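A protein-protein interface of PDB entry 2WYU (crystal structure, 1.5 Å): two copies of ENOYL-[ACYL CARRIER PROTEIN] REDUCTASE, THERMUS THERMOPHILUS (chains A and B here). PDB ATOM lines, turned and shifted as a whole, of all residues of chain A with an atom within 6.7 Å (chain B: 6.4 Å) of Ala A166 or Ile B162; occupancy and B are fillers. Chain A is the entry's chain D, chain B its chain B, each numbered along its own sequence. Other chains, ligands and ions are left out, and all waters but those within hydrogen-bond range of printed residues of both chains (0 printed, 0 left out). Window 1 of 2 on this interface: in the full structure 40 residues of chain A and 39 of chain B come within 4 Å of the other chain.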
ATOM      1  N   LEU A 118      25.372  -9.954  18.239  1.00  0.00           N
ATOM      2  CA  LEU A 118      25.594  -8.757  19.035  1.00  0.00           C
ATOM      3  C   LEU A 118      27.076  -8.434  19.170  1.00  0.00           C
ATOM      4  O   LEU A 118      27.455  -7.280  19.115  1.00  0.00           O
ATOM      5  CB  LEU A 118      24.925  -8.848  20.407  1.00  0.00           C
ATOM      6  CG  LEU A 118      23.458  -8.390  20.548  1.00  0.00           C
ATOM      7  CD1 LEU A 118      23.391  -6.884  20.528  1.00  0.00           C
ATOM      8  CD2 LEU A 118      22.526  -9.075  19.490  1.00  0.00           C
ATOM      9  N   ALA A 122      27.635  -5.107  17.078  1.00  0.00           N
ATOM     10  CA  ALA A 122      27.488  -3.961  17.979  1.00  0.00           C
ATOM     11  C   ALA A 122      28.714  -3.779  18.903  1.00  0.00           C
ATOM     12  O   ALA A 122      29.336  -2.713  18.918  1.00  0.00           O
ATOM     13  CB  ALA A 122      26.176  -4.062  18.747  1.00  0.00           C
ATOM     14  N   TYR A 123      29.114  -4.831  19.615  1.00  0.00           N
ATOM     15  CA  TYR A 123      30.272  -4.682  20.519  1.00  0.00           C
ATOM     16  C   TYR A 123      31.545  -4.263  19.749  1.00  0.00           C
ATOM     17  O   TYR A 123      32.388  -3.478  20.250  1.00  0.00           O
ATOM     18  CB  TYR A 123      30.564  -5.935  21.353  1.00  0.00           C
ATOM     19  CG  TYR A 123      31.755  -5.692  22.273  1.00  0.00           C
ATOM     20  CD1 TYR A 123      31.687  -4.804  23.351  1.00  0.00           C
ATOM     21  CD2 TYR A 123      32.985  -6.286  21.999  1.00  0.00           C
ATOM     22  CE1 TYR A 123      32.823  -4.543  24.177  1.00  0.00           C
ATOM     23  CE2 TYR A 123      34.089  -6.027  22.803  1.00  0.00           C
ATOM     24  CZ  TYR A 123      34.003  -5.170  23.856  1.00  0.00           C
ATOM     25  OH  TYR A 123      35.121  -4.942  24.601  1.00  0.00           O
ATOM     26  N   LEU A 125      31.982  -2.080  17.586  1.00  0.00           N
ATOM     27  CA  LEU A 125      32.127  -0.639  17.543  1.00  0.00           C
ATOM     28  C   LEU A 125      32.827  -0.133  18.806  1.00  0.00           C
ATOM     29  O   LEU A 125      33.689   0.742  18.727  1.00  0.00           O
ATOM     30  CB  LEU A 125      30.745   0.034  17.364  1.00  0.00           C
ATOM     31  CG  LEU A 125      30.844   1.577  17.410  1.00  0.00           C
ATOM     32  CD1 LEU A 125      31.641   2.131  16.250  1.00  0.00           C
ATOM     33  CD2 LEU A 125      29.451   2.257  17.440  1.00  0.00           C
ATOM     34  N   VAL A 126      32.450  -0.664  19.962  1.00  0.00           N
ATOM     35  CA  VAL A 126      33.059  -0.284  21.232  1.00  0.00           C
ATOM     36  C   VAL A 126      34.544  -0.685  21.252  1.00  0.00           C
ATOM     37  O   VAL A 126      35.401   0.127  21.632  1.00  0.00           O
ATOM     38  CB  VAL A 126      32.329  -0.945  22.442  1.00  0.00           C
ATOM     39  CG1 VAL A 126      33.068  -0.641  23.792  1.00  0.00           C
ATOM     40  CG2 VAL A 126      30.853  -0.499  22.467  1.00  0.00           C
ATOM     41  N   SER A 150      16.109  -1.123  13.582  1.00  0.00           N
ATOM     42  CA  SER A 150      16.387  -0.838  14.979  1.00  0.00           C
ATOM     43  C   SER A 150      15.150  -0.328  15.720  1.00  0.00           C
ATOM     44  O   SER A 150      14.972  -0.634  16.902  1.00  0.00           O
ATOM     45  CB  SER A 150      17.494   0.189  15.106  1.00  0.00           C
ATOM     46  OG  SER A 150      17.156   1.371  14.456  1.00  0.00           O
ATOM     47  N   ALA A 161      18.236  -6.537  13.768  1.00  0.00           N
ATOM     48  CA  ALA A 161      17.458  -5.359  14.236  1.00  0.00           C
ATOM     49  C   ALA A 161      17.905  -5.004  15.639  1.00  0.00           C
ATOM     50  O   ALA A 161      18.090  -3.818  15.986  1.00  0.00           O
ATOM     51  CB  ALA A 161      15.938  -5.643  14.176  1.00  0.00           C
ATOM     52  N   ILE A 162      18.011  -6.029  16.478  1.00  0.00           N
ATOM     53  CA  ILE A 162      18.390  -5.852  17.848  1.00  0.00           C
ATOM     54  C   ILE A 162      19.835  -5.396  17.931  1.00  0.00           C
ATOM     55  O   ILE A 162      20.193  -4.499  18.736  1.00  0.00           O
ATOM     56  CB  ILE A 162      18.068  -7.155  18.650  1.00  0.00           C
ATOM     57  CG1 ILE A 162      16.543  -7.254  18.938  1.00  0.00           C
ATOM     58  CG2 ILE A 162      18.811  -7.113  19.976  1.00  0.00           C
ATOM     59  CD1 ILE A 162      15.527  -7.292  17.768  1.00  0.00           C
ATOM     60  N   ALA A 163      20.704  -5.957  17.116  1.00  0.00           N
ATOM     61  CA  ALA A 163      22.065  -5.516  17.066  1.00  0.00           C
ATOM     62  C   ALA A 163      22.151  -4.044  16.642  1.00  0.00           C
ATOM     63  O   ALA A 163      22.962  -3.295  17.160  1.00  0.00           O
ATOM     64  CB  ALA A 163      22.880  -6.368  16.117  1.00  0.00           C
ATOM     65  N   LYS A 164      21.351  -3.618  15.696  1.00  0.00           N
ATOM     66  CA  LYS A 164      21.374  -2.203  15.262  1.00  0.00           C
ATOM     67  C   LYS A 164      20.845  -1.261  16.356  1.00  0.00           C
ATOM     68  O   LYS A 164      21.356  -0.153  16.508  1.00  0.00           O
ATOM     69  CB  LYS A 164      20.617  -2.042  13.930  1.00  0.00           C
ATOM     70  CG  LYS A 164      21.275  -2.750  12.726  1.00  0.00           C
ATOM     71  CD  LYS A 164      22.715  -2.392  12.513  1.00  0.00           C
ATOM     72  CE  LYS A 164      23.224  -2.822  11.125  1.00  0.00           C
ATOM     73  NZ  LYS A 164      24.687  -2.517  10.931  1.00  0.00           N
ATOM     74  N   ALA A 165      19.844  -1.695  17.128  1.00  0.00           N
ATOM     75  CA  ALA A 165      19.373  -0.920  18.271  1.00  0.00           C
ATOM     76  C   ALA A 165      20.548  -0.708  19.275  1.00  0.00           C
ATOM     77  O   ALA A 165      20.795   0.403  19.768  1.00  0.00           O
ATOM     78  CB  ALA A 165      18.173  -1.565  18.930  1.00  0.00           C
ATOM     79  N   ALA A 166      21.261  -1.788  19.572  1.00  0.00           N
ATOM     80  CA  ALA A 166      22.447  -1.727  20.446  1.00  0.00           C
ATOM     81  C   ALA A 166      23.551  -0.852  19.871  1.00  0.00           C
ATOM     82  O   ALA A 166      24.244  -0.108  20.624  1.00  0.00           O
ATOM     83  CB  ALA A 166      22.992  -3.137  20.746  1.00  0.00           C
ATOM     84  N   LEU A 167      23.733  -0.922  18.564  1.00  0.00           N
ATOM     85  CA  LEU A 167      24.737  -0.126  17.862  1.00  0.00           C
ATOM     86  C   LEU A 167      24.399   1.358  17.947  1.00  0.00           C
ATOM     87  O   LEU A 167      25.274   2.166  18.168  1.00  0.00           O
ATOM     88  CB  LEU A 167      24.804  -0.585  16.395  1.00  0.00           C
ATOM     89  CG  LEU A 167      25.819   0.062  15.478  1.00  0.00           C
ATOM     90  CD1 LEU A 167      27.280  -0.277  15.930  1.00  0.00           C
ATOM     91  CD2 LEU A 167      25.531  -0.298  13.980  1.00  0.00           C
ATOM     92  N   GLU A 168      23.141   1.729  17.711  1.00  0.00           N
ATOM     93  CA  GLU A 168      22.767   3.161  17.723  1.00  0.00           C
ATOM     94  C   GLU A 168      22.897   3.745  19.149  1.00  0.00           C
ATOM     95  O   GLU A 168      23.351   4.879  19.349  1.00  0.00           O
ATOM     96  CB  GLU A 168      21.347   3.350  17.154  1.00  0.00           C
ATOM     97  CG  GLU A 168      21.269   2.976  15.667  1.00  0.00           C
ATOM     98  CD  GLU A 168      19.897   3.104  15.051  1.00  0.00           C
ATOM     99  OE1 GLU A 168      19.002   3.741  15.644  1.00  0.00           O
ATOM    100  OE2 GLU A 168      19.706   2.535  13.932  1.00  0.00           O
ATOM    101  N   ALA A 169      22.495   2.959  20.147  1.00  0.00           N
ATOM    102  CA  ALA A 169      22.683   3.398  21.548  1.00  0.00           C
ATOM    103  C   ALA A 169      24.155   3.565  21.829  1.00  0.00           C
ATOM    104  O   ALA A 169      24.568   4.531  22.520  1.00  0.00           O
ATOM    105  CB  ALA A 169      22.042   2.404  22.515  1.00  0.00           C
ATOM    106  N   SER A 170      24.971   2.681  21.283  1.00  0.00           N
ATOM    107  CA  SER A 170      26.442   2.739  21.470  1.00  0.00           C
ATOM    108  C   SER A 170      26.980   4.013  20.838  1.00  0.00           C
ATOM    109  O   SER A 170      27.859   4.687  21.388  1.00  0.00           O
ATOM    110  CB  SER A 170      27.125   1.496  20.877  1.00  0.00           C
ATOM    111  OG  SER A 170      26.790   0.319  21.578  1.00  0.00           O
ATOM    112  N   VAL A 171      26.454   4.384  19.686  1.00  0.00           N
ATOM    113  CA  VAL A 171      26.842   5.613  19.020  1.00  0.00           C
ATOM    114  C   VAL A 171      26.611   6.826  19.933  1.00  0.00           C
ATOM    115  O   VAL A 171      27.477   7.699  20.047  1.00  0.00           O
ATOM    116  CB  VAL A 171      26.123   5.764  17.612  1.00  0.00           C
ATOM    117  CG1 VAL A 171      26.134   7.248  17.126  1.00  0.00           C
ATOM    118  CG2 VAL A 171      26.755   4.848  16.611  1.00  0.00           C
ATOM    119  N   TYR A 173      26.301   6.969  23.347  1.00  0.00           N
ATOM    120  CA  TYR A 173      27.246   6.933  24.459  1.00  0.00           C
ATOM    121  C   TYR A 173      28.677   7.252  24.043  1.00  0.00           C
ATOM    122  O   TYR A 173      29.384   8.015  24.784  1.00  0.00           O
ATOM    123  CB  TYR A 173      27.158   5.624  25.228  1.00  0.00           C
ATOM    124  CG  TYR A 173      26.079   5.631  26.249  1.00  0.00           C
ATOM    125  CD1 TYR A 173      26.397   5.823  27.584  1.00  0.00           C
ATOM    126  CD2 TYR A 173      24.728   5.480  25.900  1.00  0.00           C
ATOM    127  CE1 TYR A 173      25.429   5.866  28.551  1.00  0.00           C
ATOM    128  CE2 TYR A 173      23.721   5.516  26.899  1.00  0.00           C
ATOM    129  CZ  TYR A 173      24.121   5.716  28.228  1.00  0.00           C
ATOM    130  OH  TYR A 173      23.216   5.752  29.268  1.00  0.00           O
ATOM    131  N   TYR B 106      31.728   3.640  29.305  1.00  0.00           N
ATOM    132  CA  TYR B 106      31.173   2.655  28.410  1.00  0.00           C
ATOM    133  C   TYR B 106      32.202   2.182  27.360  1.00  0.00           C
ATOM    134  O   TYR B 106      32.299   1.000  27.069  1.00  0.00           O
ATOM    135  CB  TYR B 106      29.915   3.226  27.729  1.00  0.00           C
ATOM    136  CG  TYR B 106      29.368   2.288  26.703  1.00  0.00           C
ATOM    137  CD1 TYR B 106      28.900   1.041  27.080  1.00  0.00           C
ATOM    138  CD2 TYR B 106      29.355   2.609  25.355  1.00  0.00           C
ATOM    139  CE1 TYR B 106      28.448   0.140  26.175  1.00  0.00           C
ATOM    140  CE2 TYR B 106      28.887   1.683  24.405  1.00  0.00           C
ATOM    141  CZ  TYR B 106      28.432   0.458  24.838  1.00  0.00           C
ATOM    142  OH  TYR B 106      27.929  -0.459  23.922  1.00  0.00           O
ATOM    143  N   TRP B 114      30.425  -6.968  28.763  1.00  0.00           N
ATOM    144  CA  TRP B 114      29.396  -6.487  27.805  1.00  0.00           C
ATOM    145  C   TRP B 114      28.458  -7.611  27.371  1.00  0.00           C
ATOM    146  O   TRP B 114      27.227  -7.446  27.408  1.00  0.00           O
ATOM    147  CB  TRP B 114      30.094  -5.907  26.579  1.00  0.00           C
ATOM    148  CG  TRP B 114      29.264  -5.060  25.626  1.00  0.00           C
ATOM    149  CD1 TRP B 114      29.172  -3.709  25.615  1.00  0.00           C
ATOM    150  CD2 TRP B 114      28.453  -5.534  24.548  1.00  0.00           C
ATOM    151  NE1 TRP B 114      28.364  -3.287  24.579  1.00  0.00           N
ATOM    152  CE2 TRP B 114      27.921  -4.388  23.899  1.00  0.00           C
ATOM    153  CE3 TRP B 114      28.171  -6.795  24.018  1.00  0.00           C
ATOM    154  CZ2 TRP B 114      27.089  -4.485  22.787  1.00  0.00           C
ATOM    155  CZ3 TRP B 114      27.344  -6.877  22.936  1.00  0.00           C
ATOM    156  CH2 TRP B 114      26.827  -5.717  22.318  1.00  0.00           C
ATOM    157  N   LEU B 118      24.328  -8.050  28.199  1.00  0.00           N
ATOM    158  CA  LEU B 118      23.332  -8.223  27.140  1.00  0.00           C
ATOM    159  C   LEU B 118      22.598  -9.555  27.268  1.00  0.00           C
ATOM    160  O   LEU B 118      21.402  -9.611  27.089  1.00  0.00           O
ATOM    161  CB  LEU B 118      23.987  -8.127  25.743  1.00  0.00           C
ATOM    162  CG  LEU B 118      24.059  -6.726  25.078  1.00  0.00           C
ATOM    163  CD1 LEU B 118      22.676  -6.356  24.547  1.00  0.00           C
ATOM    164  CD2 LEU B 118      24.651  -5.658  25.994  1.00  0.00           C
ATOM    165  N   ALA B 122      18.970  -8.658  28.277  1.00  0.00           N
ATOM    166  CA  ALA B 122      18.189  -8.616  27.020  1.00  0.00           C
ATOM    167  C   ALA B 122      17.817  -9.995  26.414  1.00  0.00           C
ATOM    168  O   ALA B 122      16.649 -10.306  26.253  1.00  0.00           O
ATOM    169  CB  ALA B 122      18.875  -7.742  25.988  1.00  0.00           C
ATOM    170  N   ALA B 149      17.381   5.683  29.421  1.00  0.00           N
ATOM    171  CA  ALA B 149      18.753   5.608  28.939  1.00  0.00           C
ATOM    172  C   ALA B 149      18.919   4.810  27.639  1.00  0.00           C
ATOM    173  O   ALA B 149      19.917   4.981  26.928  1.00  0.00           O
ATOM    174  CB  ALA B 149      19.679   5.068  30.074  1.00  0.00           C
ATOM    175  N   SER B 150      17.941   3.953  27.278  1.00  0.00           N
ATOM    176  CA  SER B 150      17.949   3.324  25.951  1.00  0.00           C
ATOM    177  C   SER B 150      18.006   4.338  24.788  1.00  0.00           C
ATOM    178  O   SER B 150      18.592   4.057  23.724  1.00  0.00           O
ATOM    179  CB  SER B 150      16.711   2.456  25.769  1.00  0.00           C
ATOM    180  OG  SER B 150      15.565   3.235  25.924  1.00  0.00           O
ATOM    181  N   TYR B 157      25.226   4.785  33.377  1.00  0.00           N
ATOM    182  CA  TYR B 157      24.360   3.633  33.140  1.00  0.00           C
ATOM    183  C   TYR B 157      25.030   2.680  32.125  1.00  0.00           C
ATOM    184  O   TYR B 157      24.768   1.487  32.120  1.00  0.00           O
ATOM    185  CB  TYR B 157      22.965   4.108  32.681  1.00  0.00           C
ATOM    186  CG  TYR B 157      21.849   3.119  32.885  1.00  0.00           C
ATOM    187  CD1 TYR B 157      21.428   2.726  34.162  1.00  0.00           C
ATOM    188  CD2 TYR B 157      21.173   2.592  31.793  1.00  0.00           C
ATOM    189  CE1 TYR B 157      20.381   1.819  34.325  1.00  0.00           C
ATOM    190  CE2 TYR B 157      20.123   1.711  31.937  1.00  0.00           C
ATOM    191  CZ  TYR B 157      19.720   1.309  33.190  1.00  0.00           C
ATOM    192  OH  TYR B 157      18.680   0.404  33.288  1.00  0.00           O
ATOM    193  N   ASN B 158      25.922   3.223  31.302  1.00  0.00           N
ATOM    194  CA  ASN B 158      26.848   2.436  30.477  1.00  0.00           C
ATOM    195  C   ASN B 158      26.185   1.288  29.720  1.00  0.00           C
ATOM    196  O   ASN B 158      25.182   1.541  29.040  1.00  0.00           O
ATOM    197  CB  ASN B 158      28.046   1.976  31.332  1.00  0.00           C
ATOM    198  CG  ASN B 158      28.909   3.127  31.796  1.00  0.00           C
ATOM    199  OD1 ASN B 158      28.718   4.272  31.384  1.00  0.00           O
ATOM    200  ND2 ASN B 158      29.899   2.816  32.638  1.00  0.00           N
ATOM    201  N   VAL B 159      26.712   0.049  29.790  1.00  0.00           N
ATOM    202  CA  VAL B 159      26.156  -1.063  29.000  1.00  0.00           C
ATOM    203  C   VAL B 159      24.685  -1.334  29.327  1.00  0.00           C
ATOM    204  O   VAL B 159      23.972  -1.855  28.490  1.00  0.00           O
ATOM    205  CB  VAL B 159      26.997  -2.371  29.092  1.00  0.00           C
ATOM    206  CG1 VAL B 159      26.975  -2.937  30.541  1.00  0.00           C
ATOM    207  CG2 VAL B 159      26.510  -3.406  28.076  1.00  0.00           C
ATOM    208  N   MET B 160      24.195  -0.986  30.528  1.00  0.00           N
ATOM    209  CA  MET B 160      22.785  -1.205  30.805  1.00  0.00           C
ATOM    210  C   MET B 160      21.885  -0.413  29.838  1.00  0.00           C
ATOM    211  O   MET B 160      20.823  -0.905  29.469  1.00  0.00           O
ATOM    212  CB  MET B 160      22.419  -0.956  32.289  1.00  0.00           C
ATOM    213  CG  MET B 160      22.850  -2.060  33.250  1.00  0.00           C
ATOM    214  SD  MET B 160      22.225  -3.675  32.813  1.00  0.00           S
ATOM    215  CE  MET B 160      20.499  -3.287  32.587  1.00  0.00           C
ATOM    216  N   ALA B 161      22.321   0.754  29.391  1.00  0.00           N
ATOM    217  CA  ALA B 161      21.559   1.536  28.383  1.00  0.00           C
ATOM    218  C   ALA B 161      21.433   0.765  27.084  1.00  0.00           C
ATOM    219  O   ALA B 161      20.370   0.763  26.418  1.00  0.00           O
ATOM    220  CB  ALA B 161      22.233   2.895  28.133  1.00  0.00           C
ATOM    221  N   ILE B 162      22.551   0.167  26.693  1.00  0.00           N
ATOM    222  CA  ILE B 162      22.640  -0.589  25.480  1.00  0.00           C
ATOM    223  C   ILE B 162      21.795  -1.863  25.595  1.00  0.00           C
ATOM    224  O   ILE B 162      21.061  -2.249  24.661  1.00  0.00           O
ATOM    225  CB  ILE B 162      24.137  -0.807  25.047  1.00  0.00           C
ATOM    226  CG1 ILE B 162      24.701   0.505  24.398  1.00  0.00           C
ATOM    227  CG2 ILE B 162      24.219  -1.867  23.952  1.00  0.00           C
ATOM    228  CD1 ILE B 162      24.774   1.710  25.226  1.00  0.00           C
ATOM    229  N   ALA B 163      21.832  -2.513  26.747  1.00  0.00           N
ATOM    230  CA  ALA B 163      20.985  -3.659  27.001  1.00  0.00           C
ATOM    231  C   ALA B 163      19.502  -3.287  26.900  1.00  0.00           C
ATOM    232  O   ALA B 163      18.696  -4.060  26.380  1.00  0.00           O
ATOM    233  CB  ALA B 163      21.290  -4.309  28.396  1.00  0.00           C
ATOM    234  N   LYS B 164      19.126  -2.136  27.427  1.00  0.00           N
ATOM    235  CA  LYS B 164      17.744  -1.675  27.393  1.00  0.00           C
ATOM    236  C   LYS B 164      17.300  -1.334  25.981  1.00  0.00           C
ATOM    237  O   LYS B 164      16.159  -1.653  25.599  1.00  0.00           O
ATOM    238  CB  LYS B 164      17.523  -0.494  28.344  1.00  0.00           C
ATOM    239  CG  LYS B 164      17.628  -0.838  29.860  1.00  0.00           C
ATOM    240  CD  LYS B 164      16.844  -2.034  30.322  1.00  0.00           C
ATOM    241  CE  LYS B 164      16.779  -2.143  31.876  1.00  0.00           C
ATOM    242  NZ  LYS B 164      15.984  -3.340  32.321  1.00  0.00           N
ATOM    243  N   ALA B 165      18.186  -0.772  25.160  1.00  0.00           N
ATOM    244  CA  ALA B 165      17.866  -0.601  23.721  1.00  0.00           C
ATOM    245  C   ALA B 165      17.597  -1.946  23.069  1.00  0.00           C
ATOM    246  O   ALA B 165      16.651  -2.079  22.294  1.00  0.00           O
ATOM    247  CB  ALA B 165      18.978   0.142  23.009  1.00  0.00           C
ATOM    248  N   ALA B 166      18.437  -2.937  23.335  1.00  0.00           N
ATOM    249  CA  ALA B 166      18.250  -4.290  22.787  1.00  0.00           C
ATOM    250  C   ALA B 166      16.968  -4.936  23.301  1.00  0.00           C
ATOM    251  O   ALA B 166      16.263  -5.628  22.557  1.00  0.00           O
ATOM    252  CB  ALA B 166      19.456  -5.183  23.077  1.00  0.00           C
ATOM    253  N   LEU B 167      16.651  -4.714  24.575  1.00  0.00           N
ATOM    254  CA  LEU B 167      15.446  -5.242  25.193  1.00  0.00           C
ATOM    255  C   LEU B 167      14.174  -4.638  24.535  1.00  0.00           C
ATOM    256  O   LEU B 167      13.223  -5.354  24.217  1.00  0.00           O
ATOM    257  CB  LEU B 167      15.477  -4.904  26.697  1.00  0.00           C
ATOM    258  CG  LEU B 167      14.323  -5.394  27.565  1.00  0.00           C
ATOM    259  CD1 LEU B 167      14.373  -6.953  27.769  1.00  0.00           C
ATOM    260  CD2 LEU B 167      14.330  -4.712  28.936  1.00  0.00           C
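OH of Tyr B106 sits at hydrogen-bond distance from OG of Ser A170 (2.7 Å).
N of Tyr A123 sits at hydrogen-bond distance from O of Leu A118, 3.0 Å away.
The side-chain hydroxyl of Tyr B106 sits at hydrogen-bond distance from the indole nitrogen of Trp B114.
O of Ala A166 is in hydrogen-bond range of OG of Ser A170 (2.8 Å).
Leu A118 touches Trp B114.
Trp B114 touches Ala A122.
Ile B162 touches Ala A166.
Ala B165 touches Ala A169 (CB to CB, 3.8 Å).
Ile B162 touches Ser A170 (CG1 to OG, 3.5 Å).
Tyr A173 touches Ala B149 (OH to CB, 3.7 Å).
Tyr B157 touches Tyr A173 (CB to OH, 3.8 Å).
N of Asn B158 touches CE1 of Tyr A173, 3.8 Å away.
Tyr A173 touches Ala B161.
CD2 of Tyr A173 touches CD1 of Ile B162 (3.8 Å).
Printed residues of chain B within 4 Å of Leu A118: Trp B114 (3.6 Å).
Of the printed residues of chain B, Ala A122 touches Trp B114 (3.99 Å).
Printed residues of chain B within 4 Å of Ala A166: Ile B162 (3.7 Å).
Of the printed residues of chain B, Ser A170 touches Tyr B106 (2.7 Å) and Ile B162 (3.5 Å).
Printed residues of chain A within 4 Å of Trp B114: Leu A118 (3.6 Å), Ala A122 (3.99 Å) and Tyr A123 (3.3 Å).
Printed residues of chain A within 4 Å of Tyr B157: Tyr A173.
Leu B167 touches none of the printed residues of chain A.
The nearest residue of chain B that does not touch Ala A166 is Ala B165 (4.6 Å).
Printed residues of chain B that touch a printed residue of chain A: Tyr B106, Trp B114, Ala B149, Tyr B157, Asn B158, Ala B161, Ile B162, Ala B165 and Ala B166.
Hydrophobic or aromatic side chains of chain B within 4 Å of the printed part of chain A: Tyr B106, Trp B114, Ala B149, Tyr B157, Ala B161, Ile B162, Ala B165 and Ala B166.
Of the 18 printed residues of chain A, 10 touch a printed residue of chain B.
Among the printed residues, 17 pairs touch across the chains.
Among the printed residues, no Asp or Glu carboxylate lies within 4 Å of a Lys or Arg side-chain nitrogen of the other chain.
Ile A162 touches Ala B166, and with the chains exchanged Ala A166 touches Ile B162.
Ala B165 touches its own counterpart, Ala A165.
Positions printed for both chains: 118, 122, 150, 161, 162, 163, 164, 165, 166 and 167.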
